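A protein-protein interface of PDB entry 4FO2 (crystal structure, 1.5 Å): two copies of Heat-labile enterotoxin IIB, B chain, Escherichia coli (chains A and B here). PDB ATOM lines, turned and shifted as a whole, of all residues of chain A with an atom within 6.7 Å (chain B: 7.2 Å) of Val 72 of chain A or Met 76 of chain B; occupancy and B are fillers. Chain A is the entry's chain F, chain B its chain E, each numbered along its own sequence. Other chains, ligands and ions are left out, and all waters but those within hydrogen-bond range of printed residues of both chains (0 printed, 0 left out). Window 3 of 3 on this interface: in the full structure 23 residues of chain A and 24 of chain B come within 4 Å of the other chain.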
ATOM      1  N   LEU A  23     -24.893 -17.976  19.110  1.00  0.00           N
ATOM      2  CA  LEU A  23     -24.354 -19.280  18.645  1.00  0.00           C
ATOM      3  C   LEU A  23     -25.418 -20.046  17.857  1.00  0.00           C
ATOM      4  O   LEU A  23     -26.559 -20.242  18.358  1.00  0.00           O
ATOM      5  CB  LEU A  23     -23.909 -20.083  19.916  1.00  0.00           C
ATOM      6  CG  LEU A  23     -22.703 -19.449  20.621  1.00  0.00           C
ATOM      7  CD1 LEU A  23     -22.246 -20.380  21.808  1.00  0.00           C
ATOM      8  CD2 LEU A  23     -21.557 -19.197  19.744  1.00  0.00           C
ATOM      9  N   THR A  24     -25.111 -20.502  16.631  1.00  0.00           N
ATOM     10  CA  THR A  24     -26.153 -21.152  15.856  1.00  0.00           C
ATOM     11  C   THR A  24     -25.777 -22.545  15.464  1.00  0.00           C
ATOM     12  O   THR A  24     -26.588 -23.236  14.877  1.00  0.00           O
ATOM     13  CB  THR A  24     -26.375 -20.383  14.519  1.00  0.00           C
ATOM     14  OG1 THR A  24     -25.107 -20.270  13.838  1.00  0.00           O
ATOM     15  CG2 THR A  24     -26.942 -18.972  14.843  1.00  0.00           C
ATOM     16  N   LYS A  25     -24.521 -22.980  15.754  1.00  0.00           N
ATOM     17  CA  LYS A  25     -24.219 -24.413  15.580  1.00  0.00           C
ATOM     18  C   LYS A  25     -23.452 -24.929  16.799  1.00  0.00           C
ATOM     19  O   LYS A  25     -22.577 -24.239  17.365  1.00  0.00           O
ATOM     20  CB  LYS A  25     -23.282 -24.676  14.355  1.00  0.00           C
ATOM     21  CG  LYS A  25     -23.609 -23.760  13.088  1.00  0.00           C
ATOM     22  CD  LYS A  25     -24.577 -24.331  12.260  1.00  0.00           C
ATOM     23  CE  LYS A  25     -24.524 -23.656  10.837  1.00  0.00           C
ATOM     24  NZ  LYS A  25     -25.854 -23.697  10.280  1.00  0.00           N
ATOM     25  N   TYR A  26     -23.647 -26.231  17.005  1.00  0.00           N
ATOM     26  CA  TYR A  26     -22.963 -26.915  18.128  1.00  0.00           C
ATOM     27  C   TYR A  26     -22.472 -28.247  17.558  1.00  0.00           C
ATOM     28  O   TYR A  26     -23.233 -29.029  16.998  1.00  0.00           O
ATOM     29  CB  TYR A  26     -23.964 -27.114  19.292  1.00  0.00           C
ATOM     30  CG  TYR A  26     -23.342 -27.815  20.525  1.00  0.00           C
ATOM     31  CD1 TYR A  26     -22.383 -27.193  21.285  1.00  0.00           C
ATOM     32  CD2 TYR A  26     -23.746 -29.090  20.891  1.00  0.00           C
ATOM     33  CE1 TYR A  26     -21.859 -27.779  22.497  1.00  0.00           C
ATOM     34  CE2 TYR A  26     -23.212 -29.686  22.134  1.00  0.00           C
ATOM     35  CZ  TYR A  26     -22.245 -29.042  22.817  1.00  0.00           C
ATOM     36  OH  TYR A  26     -21.709 -29.633  23.985  1.00  0.00           O
ATOM     37  N   VAL A  39     -18.284 -24.531  18.696  1.00  0.00           N
ATOM     38  CA  VAL A  39     -19.530 -23.770  18.436  1.00  0.00           C
ATOM     39  C   VAL A  39     -19.204 -22.792  17.311  1.00  0.00           C
ATOM     40  O   VAL A  39     -18.028 -22.391  17.147  1.00  0.00           O
ATOM     41  CB  VAL A  39     -20.004 -22.973  19.674  1.00  0.00           C
ATOM     42  CG1 VAL A  39     -20.515 -23.916  20.808  1.00  0.00           C
ATOM     43  CG2 VAL A  39     -18.915 -22.055  20.280  1.00  0.00           C
ATOM     44  N   VAL A  40     -20.263 -22.424  16.548  1.00  0.00           N
ATOM     45  CA  VAL A  40     -20.147 -21.529  15.379  1.00  0.00           C
ATOM     46  C   VAL A  40     -21.139 -20.430  15.679  1.00  0.00           C
ATOM     47  O   VAL A  40     -22.316 -20.744  16.039  1.00  0.00           O
ATOM     48  CB  VAL A  40     -20.483 -22.220  14.058  1.00  0.00           C
ATOM     49  CG1 VAL A  40     -20.119 -21.277  12.851  1.00  0.00           C
ATOM     50  CG2 VAL A  40     -19.639 -23.538  13.932  1.00  0.00           C
ATOM     51  N   ILE A  67     -23.853 -24.608  28.538  1.00  0.00           N
ATOM     52  CA  ILE A  67     -24.067 -23.224  28.112  1.00  0.00           C
ATOM     53  C   ILE A  67     -24.128 -23.143  26.627  1.00  0.00           C
ATOM     54  O   ILE A  67     -25.037 -22.501  26.059  1.00  0.00           O
ATOM     55  CB  ILE A  67     -23.002 -22.295  28.677  1.00  0.00           C
ATOM     56  CG1 ILE A  67     -23.267 -22.106  30.184  1.00  0.00           C
ATOM     57  CG2 ILE A  67     -23.026 -20.826  27.996  1.00  0.00           C
ATOM     58  CD1 ILE A  67     -22.059 -21.464  30.929  1.00  0.00           C
ATOM     59  N   ALA A  68     -23.154 -23.778  25.942  1.00  0.00           N
ATOM     60  CA  ALA A  68     -23.210 -23.678  24.472  1.00  0.00           C
ATOM     61  C   ALA A  68     -24.430 -24.319  23.879  1.00  0.00           C
ATOM     62  O   ALA A  68     -25.093 -23.775  22.918  1.00  0.00           O
ATOM     63  CB  ALA A  68     -21.963 -24.337  23.871  1.00  0.00           C
ATOM     64  N   MET A  69     -24.781 -25.476  24.423  1.00  0.00           N
ATOM     65  CA  MET A  69     -25.879 -26.214  23.891  1.00  0.00           C
ATOM     66  C   MET A  69     -27.115 -25.350  24.053  1.00  0.00           C
ATOM     67  O   MET A  69     -27.876 -25.208  23.105  1.00  0.00           O
ATOM     68  CB  MET A  69     -26.085 -27.539  24.590  1.00  0.00           C
ATOM     69  CG  MET A  69     -26.968 -28.408  23.771  1.00  0.00           C
ATOM     70  SD  MET A  69     -26.376 -30.090  23.872  1.00  0.00           S
ATOM     71  CE  MET A  69     -27.183 -30.558  25.253  1.00  0.00           C
ATOM     72  N   ALA A  70     -27.264 -24.803  25.258  1.00  0.00           N
ATOM     73  CA  ALA A  70     -28.467 -24.050  25.645  1.00  0.00           C
ATOM     74  C   ALA A  70     -28.589 -22.824  24.767  1.00  0.00           C
ATOM     75  O   ALA A  70     -29.695 -22.465  24.305  1.00  0.00           O
ATOM     76  CB  ALA A  70     -28.413 -23.594  27.127  1.00  0.00           C
ATOM     77  N   ALA A  71     -27.456 -22.140  24.542  1.00  0.00           N
ATOM     78  CA  ALA A  71     -27.461 -21.000  23.608  1.00  0.00           C
ATOM     79  C   ALA A  71     -27.931 -21.386  22.233  1.00  0.00           C
ATOM     80  O   ALA A  71     -28.692 -20.629  21.597  1.00  0.00           O
ATOM     81  CB  ALA A  71     -26.043 -20.361  23.532  1.00  0.00           C
ATOM     82  N   VAL A  72     -27.474 -22.538  21.720  1.00  0.00           N
ATOM     83  CA  VAL A  72     -27.915 -22.959  20.397  1.00  0.00           C
ATOM     84  C   VAL A  72     -29.433 -23.282  20.359  1.00  0.00           C
ATOM     85  O   VAL A  72     -30.147 -22.903  19.402  1.00  0.00           O
ATOM     86  CB  VAL A  72     -27.014 -24.116  19.766  1.00  0.00           C
ATOM     87  CG1 VAL A  72     -27.654 -24.638  18.525  1.00  0.00           C
ATOM     88  CG2 VAL A  72     -25.567 -23.619  19.536  1.00  0.00           C
ATOM     89  N   LEU A  73     -29.911 -23.977  21.376  1.00  0.00           N
ATOM     90  CA  LEU A  73     -31.325 -24.386  21.430  1.00  0.00           C
ATOM     91  C   LEU A  73     -32.220 -23.189  21.700  1.00  0.00           C
ATOM     92  O   LEU A  73     -33.329 -23.165  21.161  1.00  0.00           O
ATOM     93  CB  LEU A  73     -31.596 -25.480  22.463  1.00  0.00           C
ATOM     94  CG  LEU A  73     -31.004 -26.856  22.152  1.00  0.00           C
ATOM     95  CD1 LEU A  73     -31.229 -27.775  23.384  1.00  0.00           C
ATOM     96  CD2 LEU A  73     -31.552 -27.494  20.891  1.00  0.00           C
ATOM     97  N   SER A  74     -31.771 -22.193  22.464  1.00  0.00           N
ATOM     98  CA  SER A  74     -32.716 -21.130  22.931  1.00  0.00           C
ATOM     99  C   SER A  74     -32.591 -19.814  22.189  1.00  0.00           C
ATOM    100  O   SER A  74     -33.462 -18.935  22.291  1.00  0.00           O
ATOM    101  CB  SER A  74     -32.489 -20.853  24.414  1.00  0.00           C
ATOM    102  OG  SER A  74     -31.255 -20.142  24.557  1.00  0.00           O
ATOM    103  N   GLY A  75     -31.493 -19.645  21.464  1.00  0.00           N
ATOM    104  CA  GLY A  75     -31.132 -18.387  20.896  1.00  0.00           C
ATOM    105  C   GLY A  75     -30.658 -17.342  21.895  1.00  0.00           C
ATOM    106  O   GLY A  75     -30.465 -16.177  21.507  1.00  0.00           O
ATOM    107  N   MET A  76     -30.414 -17.727  23.152  1.00  0.00           N
ATOM    108  CA  MET A  76     -29.908 -16.814  24.143  1.00  0.00           C
ATOM    109  C   MET A  76     -28.487 -16.474  23.754  1.00  0.00           C
ATOM    110  O   MET A  76     -27.819 -17.333  23.211  1.00  0.00           O
ATOM    111  CB  MET A  76     -29.928 -17.434  25.552  1.00  0.00           C
ATOM    112  CG  MET A  76     -31.306 -17.484  26.125  1.00  0.00           C
ATOM    113  SD  MET A  76     -31.212 -18.635  27.510  1.00  0.00           S
ATOM    114  CE  MET A  76     -30.714 -17.483  28.743  1.00  0.00           C
ATOM    115  N   VAL B  21     -30.460 -32.754   7.805  1.00  0.00           N
ATOM    116  CA  VAL B  21     -31.180 -33.968   8.125  1.00  0.00           C
ATOM    117  C   VAL B  21     -32.170 -33.667   9.254  1.00  0.00           C
ATOM    118  O   VAL B  21     -31.789 -33.062  10.261  1.00  0.00           O
ATOM    119  CB  VAL B  21     -30.176 -35.074   8.608  1.00  0.00           C
ATOM    120  CG1 VAL B  21     -30.880 -36.359   8.893  1.00  0.00           C
ATOM    121  CG2 VAL B  21     -29.275 -35.441   7.502  1.00  0.00           C
ATOM    122  N   GLU B  22     -33.432 -34.106   9.066  1.00  0.00           N
ATOM    123  CA  GLU B  22     -34.407 -34.047  10.136  1.00  0.00           C
ATOM    124  C   GLU B  22     -34.508 -35.383  10.803  1.00  0.00           C
ATOM    125  O   GLU B  22     -34.947 -36.319  10.226  1.00  0.00           O
ATOM    126  CB  GLU B  22     -35.793 -33.645   9.541  1.00  0.00           C
ATOM    127  CG  GLU B  22     -36.739 -33.021  10.627  1.00  0.00           C
ATOM    128  CD  GLU B  22     -38.231 -33.071  10.201  1.00  0.00           C
ATOM    129  OE1 GLU B  22     -38.482 -33.026   8.982  1.00  0.00           O
ATOM    130  OE2 GLU B  22     -39.121 -33.200  11.083  1.00  0.00           O
ATOM    131  N   LEU B  23     -34.100 -35.455  12.064  1.00  0.00           N
ATOM    132  CA  LEU B  23     -34.180 -36.722  12.796  1.00  0.00           C
ATOM    133  C   LEU B  23     -35.515 -36.832  13.551  1.00  0.00           C
ATOM    134  O   LEU B  23     -35.898 -35.889  14.230  1.00  0.00           O
ATOM    135  CB  LEU B  23     -33.038 -36.781  13.781  1.00  0.00           C
ATOM    136  CG  LEU B  23     -31.629 -36.697  13.112  1.00  0.00           C
ATOM    137  CD1 LEU B  23     -30.637 -36.660  14.352  1.00  0.00           C
ATOM    138  CD2 LEU B  23     -31.427 -37.890  12.220  1.00  0.00           C
ATOM    139  N   ILE B  67     -27.015 -34.114  21.239  1.00  0.00           N
ATOM    140  CA  ILE B  67     -27.399 -33.397  19.958  1.00  0.00           C
ATOM    141  C   ILE B  67     -28.439 -34.205  19.281  1.00  0.00           C
ATOM    142  O   ILE B  67     -29.439 -33.652  18.846  1.00  0.00           O
ATOM    143  CB  ILE B  67     -26.156 -33.224  19.034  1.00  0.00           C
ATOM    144  CG1 ILE B  67     -25.244 -32.177  19.679  1.00  0.00           C
ATOM    145  CG2 ILE B  67     -26.626 -32.846  17.570  1.00  0.00           C
ATOM    146  CD1 ILE B  67     -23.760 -32.140  19.057  1.00  0.00           C
ATOM    147  N   ALA B  68     -28.209 -35.508  19.208  1.00  0.00           N
ATOM    148  CA  ALA B  68     -29.204 -36.371  18.527  1.00  0.00           C
ATOM    149  C   ALA B  68     -30.568 -36.242  19.210  1.00  0.00           C
ATOM    150  O   ALA B  68     -31.628 -36.108  18.514  1.00  0.00           O
ATOM    151  CB  ALA B  68     -28.786 -37.787  18.570  1.00  0.00           C
ATOM    152  N   ALA B  70     -31.727 -33.930  21.271  1.00  0.00           N
ATOM    153  CA  ALA B  70     -32.277 -32.577  21.130  1.00  0.00           C
ATOM    154  C   ALA B  70     -32.869 -32.316  19.787  1.00  0.00           C
ATOM    155  O   ALA B  70     -33.863 -31.596  19.691  1.00  0.00           O
ATOM    156  CB  ALA B  70     -31.169 -31.482  21.435  1.00  0.00           C
ATOM    157  N   ALA B  71     -32.266 -32.843  18.727  1.00  0.00           N
ATOM    158  CA  ALA B  71     -32.784 -32.648  17.376  1.00  0.00           C
ATOM    159  C   ALA B  71     -34.159 -33.361  17.247  1.00  0.00           C
ATOM    160  O   ALA B  71     -35.104 -32.860  16.600  1.00  0.00           O
ATOM    161  CB  ALA B  71     -31.723 -33.263  16.343  1.00  0.00           C
ATOM    162  N   VAL B  72     -34.260 -34.540  17.874  1.00  0.00           N
ATOM    163  CA  VAL B  72     -35.514 -35.337  17.720  1.00  0.00           C
ATOM    164  C   VAL B  72     -36.605 -34.601  18.479  1.00  0.00           C
ATOM    165  O   VAL B  72     -37.707 -34.374  17.910  1.00  0.00           O
ATOM    166  CB  VAL B  72     -35.338 -36.722  18.215  1.00  0.00           C
ATOM    167  CG1 VAL B  72     -36.721 -37.414  18.490  1.00  0.00           C
ATOM    168  CG2 VAL B  72     -34.553 -37.582  17.208  1.00  0.00           C
ATOM    169  N   LEU B  73     -36.294 -34.121  19.687  1.00  0.00           N
ATOM    170  CA  LEU B  73     -37.289 -33.328  20.511  1.00  0.00           C
ATOM    171  C   LEU B  73     -37.702 -31.989  19.875  1.00  0.00           C
ATOM    172  O   LEU B  73     -38.896 -31.609  19.929  1.00  0.00           O
ATOM    173  CB  LEU B  73     -36.813 -33.120  21.976  1.00  0.00           C
ATOM    174  CG  LEU B  73     -36.746 -34.400  22.865  1.00  0.00           C
ATOM    175  CD1 LEU B  73     -35.880 -34.242  24.163  1.00  0.00           C
ATOM    176  CD2 LEU B  73     -38.127 -34.912  23.239  1.00  0.00           C
ATOM    177  N   SER B  74     -36.791 -31.324  19.190  1.00  0.00           N
ATOM    178  CA  SER B  74     -37.044 -29.955  18.760  1.00  0.00           C
ATOM    179  C   SER B  74     -37.425 -29.784  17.286  1.00  0.00           C
ATOM    180  O   SER B  74     -38.031 -28.731  16.917  1.00  0.00           O
ATOM    181  CB  SER B  74     -35.857 -29.086  19.103  1.00  0.00           C
ATOM    182  OG  SER B  74     -34.791 -29.371  18.194  1.00  0.00           O
ATOM    183  N   GLY B  75     -37.072 -30.779  16.465  1.00  0.00           N
ATOM    184  CA  GLY B  75     -37.091 -30.746  15.008  1.00  0.00           C
ATOM    185  C   GLY B  75     -35.991 -29.908  14.371  1.00  0.00           C
ATOM    186  O   GLY B  75     -36.034 -29.612  13.177  1.00  0.00           O
ATOM    187  N   MET B  76     -35.009 -29.480  15.169  1.00  0.00           N
ATOM    188  CA  MET B  76     -33.828 -28.787  14.664  1.00  0.00           C
ATOM    189  C   MET B  76     -33.054 -29.749  13.769  1.00  0.00           C
ATOM    190  O   MET B  76     -32.986 -30.976  14.048  1.00  0.00           O
ATOM    191  CB  MET B  76     -32.951 -28.380  15.843  1.00  0.00           C
ATOM    192  CG  MET B  76     -33.511 -27.157  16.570  1.00  0.00           C
ATOM    193  SD  MET B  76     -32.293 -26.687  17.804  1.00  0.00           S
ATOM    194  CE  MET B  76     -32.709 -24.923  17.901  1.00  0.00           C
ATOM    195  N   ARG B  77     -32.493 -29.225  12.689  1.00  0.00           N
ATOM    196  CA  ARG B  77     -31.843 -30.109  11.721  1.00  0.00           C
ATOM    197  C   ARG B  77     -30.403 -30.398  12.178  1.00  0.00           C
ATOM    198  O   ARG B  77     -29.859 -29.605  12.881  1.00  0.00           O
ATOM    199  CB  ARG B  77     -31.734 -29.449  10.366  1.00  0.00           C
ATOM    200  CG  ARG B  77     -33.122 -29.017   9.759  1.00  0.00           C
ATOM    201  CD  ARG B  77     -33.914 -30.122   9.168  1.00  0.00           C
ATOM    202  NE  ARG B  77     -34.385 -29.689   7.851  1.00  0.00           N
ATOM    203  CZ  ARG B  77     -35.582 -29.948   7.310  1.00  0.00           C
ATOM    204  NH1 ARG B  77     -36.514 -30.640   7.964  1.00  0.00           N
ATOM    205  NH2 ARG B  77     -35.846 -29.483   6.089  1.00  0.00           N
ATOM    206  N   VAL B  78     -29.808 -31.482  11.676  1.00  0.00           N
ATOM    207  CA  VAL B  78     -28.380 -31.693  11.967  1.00  0.00           C
ATOM    208  C   VAL B  78     -27.639 -31.897  10.652  1.00  0.00           C
ATOM    209  O   VAL B  78     -28.231 -32.280   9.660  1.00  0.00           O
ATOM    210  CB  VAL B  78     -28.197 -32.949  12.850  1.00  0.00           C
ATOM    211  CG1 VAL B  78     -28.904 -32.642  14.220  1.00  0.00           C
ATOM    212  CG2 VAL B  78     -28.672 -34.208  12.212  1.00  0.00           C
ATOM    213  N   LEU B  96     -25.403 -29.627  15.306  1.00  0.00           N
ATOM    214  CA  LEU B  96     -26.813 -29.258  15.564  1.00  0.00           C
ATOM    215  C   LEU B  96     -26.975 -27.825  15.089  1.00  0.00           C
ATOM    216  O   LEU B  96     -26.157 -26.960  15.357  1.00  0.00           O
ATOM    217  CB  LEU B  96     -26.962 -29.231  17.074  1.00  0.00           C
ATOM    218  CG  LEU B  96     -28.375 -28.775  17.494  1.00  0.00           C
ATOM    219  CD1 LEU B  96     -29.387 -29.785  16.985  1.00  0.00           C
ATOM    220  CD2 LEU B  96     -28.393 -28.757  19.032  1.00  0.00           C
ATOM    221  N   GLU B  97     -28.038 -27.554  14.323  1.00  0.00           N
ATOM    222  CA  GLU B  97     -28.174 -26.148  13.936  1.00  0.00           C
ATOM    223  C   GLU B  97     -29.483 -25.576  14.410  1.00  0.00           C
ATOM    224  O   GLU B  97     -30.528 -26.220  14.322  1.00  0.00           O
ATOM    225  CB  GLU B  97     -27.928 -25.818  12.427  1.00  0.00           C
ATOM    226  CG  GLU B  97     -28.018 -26.906  11.504  1.00  0.00           C
ATOM    227  CD  GLU B  97     -28.173 -26.496  10.037  1.00  0.00           C
ATOM    228  OE1 GLU B  97     -27.148 -26.260   9.341  1.00  0.00           O
ATOM    229  OE2 GLU B  97     -29.336 -26.500   9.570  1.00  0.00           O
ATOM    230  N   ALA B  98     -29.381 -24.338  14.856  1.00  0.00           N
ATOM    231  CA  ALA B  98     -30.494 -23.591  15.442  1.00  0.00           C
ATOM    232  C   ALA B  98     -31.470 -23.315  14.287  1.00  0.00           C
ATOM    233  O   ALA B  98     -31.017 -22.980  13.182  1.00  0.00           O
ATOM    234  CB  ALA B  98     -29.976 -22.275  16.042  1.00  0.00           C
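Printed residues of chain B that touch a printed residue of chain A: Ile 67, Met 76, Leu 96, Glu 97 and Ala 98.
Hydrophobic or aromatic side chains of chain B that line the printed part of chain A: Ile 67, Met 76, Leu 96 and Ala 98.
Along chain B the printed residues that touch a printed residue of chain A span positions 67 to 98.
Of the 16 printed residues of chain A, 5 touch a printed residue of chain B.
Hydrophobic or aromatic side chains of chain A within 4 Å of the printed part of chain B: Tyr 26 and Leu 73.
O of Tyr 26 of chain A is in hydrogen-bond range of N of Leu 96 of chain B.
The side-chain carboxylate (OE1) of Glu 97 of chain B lies within salt-bridge range of the side-chain amino group (NZ) of Lys 25 of chain A (3.0 Å).
N of Ala 98 of chain B lies within hydrogen-bond range of O of Thr 24 of chain A (3.0 Å).
O of Thr 24 of chain A touches O of Leu 96 of chain B, at 3.8 Å.
O of Thr 24 of chain A touches CA of Glu 97 of chain B, at 3.4 Å.
Lys 25 of chain A touches Leu 96 of chain B (CA to O, 3.2 Å).
Ile 67 of chain B touches Tyr 26 of chain A.
Val 72 of chain A touches Met 76 of chain B.
O of Val 72 of chain A touches CB of Ala 98 of chain B (3.4 Å).
Leu 73 of chain A touches Met 76 of chain B (CD2 to SD, 3.3 Å).
Leu 73 of chain A touches Leu 96 of chain B (CD2 to CD2, 3.9 Å).
The backbone NH (N) of Val 40 of chain A is in hydrogen-bond range of the backbone carbonyl oxygen (O) of Lys 25 of chain A.
The side-chain hydroxyl (OG) of Ser 74 of chain B sits close to the backbone NH (N) of Met 76 of chain B, 3.0 Å away.
N of Glu 97 of chain B sits at hydrogen-bond distance from O of Arg 77 of chain B.
N of Thr 24 of chain A lies within hydrogen-bond range of O of Val 40 of chain A, at 2.9 Å.
Val 72 of chain A touches two residues of chain B.
Of the printed residues of chain B, Thr 24 of chain A touches Leu 96 (3.8 Å), Glu 97 (3.4 Å) and Ala 98 (3.0 Å).
Printed residues of chain A within 4 Å of Ile 67 of chain B: Tyr 26.
Printed residues of chain A within 4 Å of Ala 98 of chain B: Thr 24 (3.0 Å) and Val 72 (3.4 Å).
Printed residues of chain B within 4 Å of Leu 73 of chain A: Met 76 and Leu 96.
Gly 75 of chain B touches none of the printed residues of chain A.
Val 72 of chain B touches none of the printed residues of chain A.
The nearest printed residue of chain B that does not touch Lys 25 of chain A is Ala 98 of chain B (5.1 Å).
Val 72 of chain A touches Met 76 of chain B, but with the chains exchanged Met 76 of chain A does not touch Val 72 of chain B (18.0 Å).
Leu 73 of chain A touches Met 76 of chain B, but with the chains exchanged Met 76 of chain A does not touch Leu 73 of chain B (16.3 Å).
Positions printed for both chains: 23, 67, 68, 70, 71, 72, 73, 74, 75 and 76.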
